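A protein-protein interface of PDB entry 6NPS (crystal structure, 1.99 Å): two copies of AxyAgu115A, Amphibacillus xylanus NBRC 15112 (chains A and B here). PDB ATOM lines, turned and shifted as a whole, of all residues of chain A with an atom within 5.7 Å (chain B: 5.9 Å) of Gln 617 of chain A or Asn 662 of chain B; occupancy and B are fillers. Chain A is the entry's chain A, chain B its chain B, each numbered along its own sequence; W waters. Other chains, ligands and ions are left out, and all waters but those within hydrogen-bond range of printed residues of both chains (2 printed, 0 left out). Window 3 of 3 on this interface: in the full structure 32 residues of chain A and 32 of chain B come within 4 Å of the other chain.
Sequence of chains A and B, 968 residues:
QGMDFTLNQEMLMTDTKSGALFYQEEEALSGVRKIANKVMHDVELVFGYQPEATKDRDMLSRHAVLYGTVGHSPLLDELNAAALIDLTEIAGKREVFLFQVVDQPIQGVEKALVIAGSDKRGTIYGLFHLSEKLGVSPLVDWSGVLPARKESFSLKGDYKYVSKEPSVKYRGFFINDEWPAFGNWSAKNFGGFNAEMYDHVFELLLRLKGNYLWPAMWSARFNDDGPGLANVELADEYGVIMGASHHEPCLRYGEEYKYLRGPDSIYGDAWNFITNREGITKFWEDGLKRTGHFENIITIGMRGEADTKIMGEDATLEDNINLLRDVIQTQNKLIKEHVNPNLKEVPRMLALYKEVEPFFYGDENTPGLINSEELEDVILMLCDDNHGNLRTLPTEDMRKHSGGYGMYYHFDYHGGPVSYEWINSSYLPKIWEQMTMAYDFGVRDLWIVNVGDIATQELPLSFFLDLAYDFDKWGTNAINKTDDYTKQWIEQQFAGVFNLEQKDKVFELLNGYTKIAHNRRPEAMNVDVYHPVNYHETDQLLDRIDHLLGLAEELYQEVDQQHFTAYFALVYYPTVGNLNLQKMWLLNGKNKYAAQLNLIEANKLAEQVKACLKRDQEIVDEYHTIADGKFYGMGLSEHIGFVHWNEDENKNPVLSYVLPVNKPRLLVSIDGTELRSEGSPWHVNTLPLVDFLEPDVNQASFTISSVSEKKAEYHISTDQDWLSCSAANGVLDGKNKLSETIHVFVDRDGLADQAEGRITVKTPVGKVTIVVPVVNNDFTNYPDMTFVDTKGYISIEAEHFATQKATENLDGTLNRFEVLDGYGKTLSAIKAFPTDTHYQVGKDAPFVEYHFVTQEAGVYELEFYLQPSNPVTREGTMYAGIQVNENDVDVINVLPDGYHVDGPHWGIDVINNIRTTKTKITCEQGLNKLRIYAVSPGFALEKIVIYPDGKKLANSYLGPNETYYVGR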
ATOM      1  N   CYS A 612      -4.099 -17.501 -28.763  1.00  0.00           N
ATOM      2  CA  CYS A 612      -3.087 -16.502 -29.131  1.00  0.00           C
ATOM      3  C   CYS A 612      -3.549 -15.100 -28.793  1.00  0.00           C
ATOM      4  O   CYS A 612      -2.763 -14.257 -28.302  1.00  0.00           O
ATOM      5  CB  CYS A 612      -2.772 -16.586 -30.629  1.00  0.00           C
ATOM      6  SG  CYS A 612      -1.777 -18.024 -31.037  1.00  0.00           S
ATOM      7  N   LEU A 613      -4.800 -14.795 -29.088  1.00  0.00           N
ATOM      8  CA  LEU A 613      -5.281 -13.455 -28.773  1.00  0.00           C
ATOM      9  C   LEU A 613      -5.256 -13.190 -27.266  1.00  0.00           C
ATOM     10  O   LEU A 613      -4.919 -12.084 -26.818  1.00  0.00           O
ATOM     11  CB  LEU A 613      -6.694 -13.268 -29.337  1.00  0.00           C
ATOM     12  CG  LEU A 613      -7.200 -11.831 -29.206  1.00  0.00           C
ATOM     13  CD1 LEU A 613      -6.328 -10.941 -30.087  1.00  0.00           C
ATOM     14  CD2 LEU A 613      -8.638 -11.743 -29.648  1.00  0.00           C
ATOM     15  N   LYS A 614      -5.633 -14.185 -26.472  1.00  0.00           N
ATOM     16  CA  LYS A 614      -5.534 -14.043 -25.025  1.00  0.00           C
ATOM     17  C   LYS A 614      -4.087 -13.827 -24.576  1.00  0.00           C
ATOM     18  O   LYS A 614      -3.809 -12.997 -23.689  1.00  0.00           O
ATOM     19  CB  LYS A 614      -6.113 -15.285 -24.365  1.00  0.00           C
ATOM     20  CG  LYS A 614      -6.130 -15.281 -22.853  1.00  0.00           C
ATOM     21  CD  LYS A 614      -7.059 -16.410 -22.366  1.00  0.00           C
ATOM     22  CE  LYS A 614      -6.765 -16.827 -20.920  1.00  0.00           C
ATOM     23  NZ  LYS A 614      -6.510 -18.304 -20.755  1.00  0.00           N
ATOM     24  N   ARG A 615      -3.143 -14.562 -25.175  1.00  0.00           N
ATOM     25  CA  ARG A 615      -1.746 -14.401 -24.781  1.00  0.00           C
ATOM     26  C   ARG A 615      -1.218 -13.013 -25.142  1.00  0.00           C
ATOM     27  O   ARG A 615      -0.364 -12.476 -24.431  1.00  0.00           O
ATOM     28  CB  ARG A 615      -0.895 -15.511 -25.420  1.00  0.00           C
ATOM     29  CG  ARG A 615       0.608 -15.352 -25.211  1.00  0.00           C
ATOM     30  CD  ARG A 615       1.105 -16.012 -23.915  1.00  0.00           C
ATOM     31  NE  ARG A 615       2.563 -15.966 -23.860  1.00  0.00           N
ATOM     32  CZ  ARG A 615       3.279 -15.466 -22.859  1.00  0.00           C
ATOM     33  NH1 ARG A 615       2.729 -15.186 -21.701  1.00  0.00           N
ATOM     34  NH2 ARG A 615       4.561 -15.260 -23.030  1.00  0.00           N
ATOM     35  N   ASP A 616      -1.722 -12.403 -26.217  1.00  0.00           N
ATOM     36  CA  ASP A 616      -1.295 -11.045 -26.563  1.00  0.00           C
ATOM     37  C   ASP A 616      -1.643 -10.050 -25.453  1.00  0.00           C
ATOM     38  O   ASP A 616      -0.851  -9.157 -25.129  1.00  0.00           O
ATOM     39  CB  ASP A 616      -1.942 -10.598 -27.881  1.00  0.00           C
ATOM     40  CG  ASP A 616      -1.679  -9.111 -28.187  1.00  0.00           C
ATOM     41  OD1 ASP A 616      -0.646  -8.801 -28.826  1.00  0.00           O
ATOM     42  OD2 ASP A 616      -2.508  -8.259 -27.787  1.00  0.00           O
ATOM     43  N   GLN A 617      -2.826 -10.179 -24.872  1.00  0.00           N
ATOM     44  CA  GLN A 617      -3.171  -9.263 -23.811  1.00  0.00           C
ATOM     45  C   GLN A 617      -2.414  -9.588 -22.530  1.00  0.00           C
ATOM     46  O   GLN A 617      -2.090  -8.676 -21.760  1.00  0.00           O
ATOM     47  CB  GLN A 617      -4.683  -9.278 -23.583  1.00  0.00           C
ATOM     48  CG  GLN A 617      -5.191  -7.987 -22.946  1.00  0.00           C
ATOM     49  CD  GLN A 617      -4.402  -6.741 -23.382  1.00  0.00           C
ATOM     50  OE1 GLN A 617      -4.627  -6.198 -24.471  1.00  0.00           O
ATOM     51  NE2 GLN A 617      -3.487  -6.275 -22.522  1.00  0.00           N
ATOM     52  N   GLU A 618      -2.106 -10.861 -22.293  1.00  0.00           N
ATOM     53  CA  GLU A 618      -1.377 -11.218 -21.084  1.00  0.00           C
ATOM     54  C   GLU A 618       0.046 -10.701 -21.130  1.00  0.00           C
ATOM     55  O   GLU A 618       0.548 -10.199 -20.124  1.00  0.00           O
ATOM     56  CB  GLU A 618      -1.390 -12.722 -20.867  1.00  0.00           C
ATOM     57  CG  GLU A 618      -2.719 -13.188 -20.328  1.00  0.00           C
ATOM     58  CD  GLU A 618      -2.827 -14.693 -20.216  1.00  0.00           C
ATOM     59  OE1 GLU A 618      -1.908 -15.394 -20.702  1.00  0.00           O
ATOM     60  OE2 GLU A 618      -3.847 -15.172 -19.660  1.00  0.00           O
ATOM     61  N   ILE A 619       0.708 -10.802 -22.281  1.00  0.00           N
ATOM     62  CA  ILE A 619       2.095 -10.383 -22.317  1.00  0.00           C
ATOM     63  C   ILE A 619       2.216  -8.857 -22.207  1.00  0.00           C
ATOM     64  O   ILE A 619       3.178  -8.359 -21.621  1.00  0.00           O
ATOM     65  CB  ILE A 619       2.775 -10.926 -23.575  1.00  0.00           C
ATOM     66  CG1 ILE A 619       4.279 -10.900 -23.374  1.00  0.00           C
ATOM     67  CG2 ILE A 619       2.358 -10.146 -24.825  1.00  0.00           C
ATOM     68  CD1 ILE A 619       5.031 -11.145 -24.626  1.00  0.00           C
ATOM     69  N   VAL A 620       1.242  -8.099 -22.737  1.00  0.00           N
ATOM     70  CA  VAL A 620       1.251  -6.640 -22.575  1.00  0.00           C
ATOM     71  C   VAL A 620       1.061  -6.265 -21.111  1.00  0.00           C
ATOM     72  O   VAL A 620       1.781  -5.399 -20.577  1.00  0.00           O
ATOM     73  CB  VAL A 620       0.172  -5.984 -23.465  1.00  0.00           C
ATOM     74  CG1 VAL A 620      -0.016  -4.510 -23.103  1.00  0.00           C
ATOM     75  CG2 VAL A 620       0.517  -6.137 -24.955  1.00  0.00           C
ATOM     76  N   ASP A 621       0.086  -6.891 -20.443  1.00  0.00           N
ATOM     77  CA  ASP A 621      -0.136  -6.618 -19.026  1.00  0.00           C
ATOM     78  C   ASP A 621       1.102  -6.925 -18.205  1.00  0.00           C
ATOM     79  O   ASP A 621       1.460  -6.157 -17.297  1.00  0.00           O
ATOM     80  CB  ASP A 621      -1.315  -7.430 -18.497  1.00  0.00           C
ATOM     81  CG  ASP A 621      -2.635  -6.959 -19.056  1.00  0.00           C
ATOM     82  OD1 ASP A 621      -3.518  -7.811 -19.304  1.00  0.00           O
ATOM     83  OD2 ASP A 621      -2.778  -5.730 -19.255  1.00  0.00           O
ATOM     84  N   GLU A 622       1.752  -8.067 -18.482  1.00  0.00           N
ATOM     85  CA  GLU A 622       2.996  -8.387 -17.790  1.00  0.00           C
ATOM     86  C   GLU A 622       4.046  -7.306 -18.035  1.00  0.00           C
ATOM     87  O   GLU A 622       4.726  -6.865 -17.102  1.00  0.00           O
ATOM     88  CB  GLU A 622       3.503  -9.779 -18.215  1.00  0.00           C
ATOM     89  CG  GLU A 622       4.770 -10.229 -17.467  1.00  0.00           C
ATOM     90  CD  GLU A 622       5.127 -11.743 -17.646  1.00  0.00           C
ATOM     91  OE1 GLU A 622       4.526 -12.426 -18.521  1.00  0.00           O
ATOM     92  OE2 GLU A 622       6.023 -12.236 -16.896  1.00  0.00           O
ATOM     93  N   GLU A 638      -2.809   0.088 -29.955  1.00  0.00           N
ATOM     94  CA  GLU A 638      -3.553  -0.875 -30.764  1.00  0.00           C
ATOM     95  C   GLU A 638      -2.656  -1.361 -31.875  1.00  0.00           C
ATOM     96  O   GLU A 638      -1.988  -0.562 -32.537  1.00  0.00           O
ATOM     97  CB  GLU A 638      -4.808  -0.246 -31.380  1.00  0.00           C
ATOM     98  CG  GLU A 638      -5.930   0.012 -30.404  1.00  0.00           C
ATOM     99  CD  GLU A 638      -6.409  -1.266 -29.746  1.00  0.00           C
ATOM    100  OE1 GLU A 638      -6.638  -2.258 -30.470  1.00  0.00           O
ATOM    101  OE2 GLU A 638      -6.536  -1.280 -28.503  1.00  0.00           O
ATOM    102  N   ASN A 652     -10.275  -7.810 -34.960  1.00  0.00           N
ATOM    103  CA  ASN A 652      -9.677  -9.072 -34.546  1.00  0.00           C
ATOM    104  C   ASN A 652      -9.889 -10.169 -35.601  1.00  0.00           C
ATOM    105  O   ASN A 652     -10.729 -10.030 -36.503  1.00  0.00           O
ATOM    106  CB  ASN A 652     -10.292  -9.487 -33.210  1.00  0.00           C
ATOM    107  CG  ASN A 652      -9.628  -8.801 -32.043  1.00  0.00           C
ATOM    108  OD1 ASN A 652      -8.465  -8.427 -32.136  1.00  0.00           O
ATOM    109  ND2 ASN A 652     -10.356  -8.626 -30.948  1.00  0.00           N
ATOM    110  N   PRO B 660     -14.022  -9.931 -29.127  1.00  0.00           N
ATOM    111  CA  PRO B 660     -14.225  -8.488 -28.866  1.00  0.00           C
ATOM    112  C   PRO B 660     -12.947  -7.667 -28.981  1.00  0.00           C
ATOM    113  O   PRO B 660     -11.866  -8.087 -28.569  1.00  0.00           O
ATOM    114  CB  PRO B 660     -14.757  -8.459 -27.420  1.00  0.00           C
ATOM    115  CG  PRO B 660     -15.322  -9.848 -27.196  1.00  0.00           C
ATOM    116  CD  PRO B 660     -14.501 -10.797 -28.032  1.00  0.00           C
ATOM    117  N   VAL B 661     -13.078  -6.434 -29.476  1.00  0.00           N
ATOM    118  CA  VAL B 661     -11.886  -5.577 -29.496  1.00  0.00           C
ATOM    119  C   VAL B 661     -11.713  -4.891 -28.141  1.00  0.00           C
ATOM    120  O   VAL B 661     -12.586  -4.969 -27.271  1.00  0.00           O
ATOM    121  CB  VAL B 661     -11.959  -4.530 -30.626  1.00  0.00           C
ATOM    122  CG1 VAL B 661     -12.022  -5.224 -31.990  1.00  0.00           C
ATOM    123  CG2 VAL B 661     -13.174  -3.634 -30.418  1.00  0.00           C
ATOM    124  N   ASN B 662     -10.588  -4.200 -27.973  1.00  0.00           N
ATOM    125  CA  ASN B 662     -10.216  -3.588 -26.701  1.00  0.00           C
ATOM    126  C   ASN B 662     -10.967  -2.291 -26.432  1.00  0.00           C
ATOM    127  O   ASN B 662     -11.400  -2.057 -25.300  1.00  0.00           O
ATOM    128  CB  ASN B 662      -8.710  -3.330 -26.677  1.00  0.00           C
ATOM    129  CG  ASN B 662      -7.893  -4.622 -26.737  1.00  0.00           C
ATOM    130  OD1 ASN B 662      -8.349  -5.669 -26.287  1.00  0.00           O
ATOM    131  ND2 ASN B 662      -6.676  -4.541 -27.278  1.00  0.00           N
ATOM    132  N   LYS B 663     -11.147  -1.411 -27.470  1.00  0.00           N
ATOM    133  CA  LYS B 663     -11.698  -0.110 -27.064  1.00  0.00           C
ATOM    134  C   LYS B 663     -13.221  -0.095 -27.106  1.00  0.00           C
ATOM    135  O   LYS B 663     -13.827  -0.812 -27.910  1.00  0.00           O
ATOM    136  CB  LYS B 663     -11.174   0.990 -27.975  1.00  0.00           C
ATOM    137  CG  LYS B 663      -9.786   1.428 -27.627  1.00  0.00           C
ATOM    138  CD  LYS B 663      -9.334   2.534 -28.534  1.00  0.00           C
ATOM    139  CE  LYS B 663      -7.820   2.667 -28.425  1.00  0.00           C
ATOM    140  NZ  LYS B 663      -7.302   3.864 -29.132  1.00  0.00           N
ATOM    141  N   PRO B 664     -13.882   0.761 -26.276  1.00  0.00           N
ATOM    142  CA  PRO B 664     -15.360   0.801 -26.266  1.00  0.00           C
ATOM    143  C   PRO B 664     -15.982   1.516 -27.466  1.00  0.00           C
ATOM    144  O   PRO B 664     -16.612   2.580 -27.346  1.00  0.00           O
ATOM    145  CB  PRO B 664     -15.673   1.535 -24.955  1.00  0.00           C
ATOM    146  CG  PRO B 664     -14.515   2.420 -24.749  1.00  0.00           C
ATOM    147  CD  PRO B 664     -13.306   1.652 -25.246  1.00  0.00           C
ATOM    148  N   ARG B 665     -15.819   0.911 -28.625  1.00  0.00           N
ATOM    149  CA  ARG B 665     -16.237   1.448 -29.903  1.00  0.00           C
ATOM    150  C   ARG B 665     -17.668   1.027 -30.209  1.00  0.00           C
ATOM    151  O   ARG B 665     -18.150  -0.010 -29.736  1.00  0.00           O
ATOM    152  CB  ARG B 665     -15.296   0.951 -31.016  1.00  0.00           C
ATOM    153  CG  ARG B 665     -13.822   1.268 -30.732  1.00  0.00           C
ATOM    154  CD  ARG B 665     -12.825   0.265 -31.386  1.00  0.00           C
ATOM    155  NE  ARG B 665     -13.373  -0.251 -32.632  1.00  0.00           N
ATOM    156  CZ  ARG B 665     -12.749  -1.105 -33.426  1.00  0.00           C
ATOM    157  NH1 ARG B 665     -11.540  -1.534 -33.054  1.00  0.00           N
ATOM    158  NH2 ARG B 665     -13.359  -1.561 -34.532  1.00  0.00           N
ATOM    159  N   SER B 708     -17.093  -4.367 -28.703  1.00  0.00           N
ATOM    160  CA  SER B 708     -16.304  -4.760 -27.553  1.00  0.00           C
ATOM    161  C   SER B 708     -17.240  -5.224 -26.446  1.00  0.00           C
ATOM    162  O   SER B 708     -18.458  -5.023 -26.504  1.00  0.00           O
ATOM    163  CB  SER B 708     -15.457  -3.600 -27.037  1.00  0.00           C
ATOM    164  OG  SER B 708     -16.298  -2.768 -26.266  1.00  0.00           O
ATOM    165  N   LYS B 710     -16.896  -3.818 -23.532  1.00  0.00           N
ATOM    166  CA  LYS B 710     -16.811  -2.673 -22.640  1.00  0.00           C
ATOM    167  C   LYS B 710     -18.161  -1.955 -22.594  1.00  0.00           C
ATOM    168  O   LYS B 710     -18.935  -1.979 -23.556  1.00  0.00           O
ATOM    169  CB  LYS B 710     -15.727  -1.693 -23.111  1.00  0.00           C
ATOM    170  CG  LYS B 710     -14.369  -1.851 -22.448  1.00  0.00           C
ATOM    171  CD  LYS B 710     -13.869  -3.273 -22.537  1.00  0.00           C
ATOM    172  CE  LYS B 710     -12.461  -3.406 -21.971  1.00  0.00           C
ATOM    173  NZ  LYS B 710     -11.391  -3.287 -23.001  1.00  0.00           N
HETATM  174  O   HOH W   1      -8.507  -4.189 -30.439  1.00  0.00           O
HETATM  175  O   HOH W   2      -9.872  -1.249 -30.233  1.00  0.00           O
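OD2 of Asp 621 of chain A is in hydrogen-bond range of NE2 of Gln 617 of chain A (3.4 Å). NZ of Lys 710 of chain B lies within hydrogen-bond range of O of Asn 662 of chain B.
Water W1 bridges the side-chain carboxylate of Glu 638 of chain A (2.7 Å) and the backbone NH of Asn 662 of chain B (3.2 Å). Water W2 lies within hydrogen-bond range of N of Lys 663 of chain B (3.0 Å), NH1 of Arg 665 of chain B (3.3 Å) and OE1 of Glu 638 of chain A (3.4 Å).
Among the printed residues, merely in contact across the chains: Asn 652 of chain A with Val 661 of chain B (3.7 Å), Glu 638 of chain A with Lys 663 of chain B (3.8 Å) and Gln 617 of chain A with Asn 662 of chain B (3.9 Å).
Among the printed residues, no Asp or Glu carboxylate lies within 4 Å of a Lys or Arg side-chain nitrogen of the other chain.
The side-chain carboxylate (OE2) of Glu 638 of chain A is in hydrogen-bond range of the side-chain amide nitrogen (ND2) of Asn 662 of chain B (3.5 Å). O of Pro 660 of chain B lies within hydrogen-bond range of ND2 of Asn 652 of chain A, 2.9 Å away.
Of the printed residues of chain B, Gln 617 of chain A touches Asn 662. Printed residues of chain A within 4 Å of Pro 660 of chain B: Asn 652. Printed residues of chain A within 4 Å of Val 661 of chain B: Asn 652 (3.7 Å). Of the printed residues of chain B, Asn 652 of chain A touches Pro 660 and Val 661. Of the printed residues of chain A, Lys 663 of chain B touches Glu 638 (3.8 Å). Of the printed residues of chain B, Glu 638 of chain A touches Asn 662 and Lys 663. Glu 622 of chain A touches none of the printed residues of chain B. The nearest residue of chain A that does not touch Asn 662 of chain B is Asn 652 of chain A (5.3 Å).
No position is printed for both chains.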
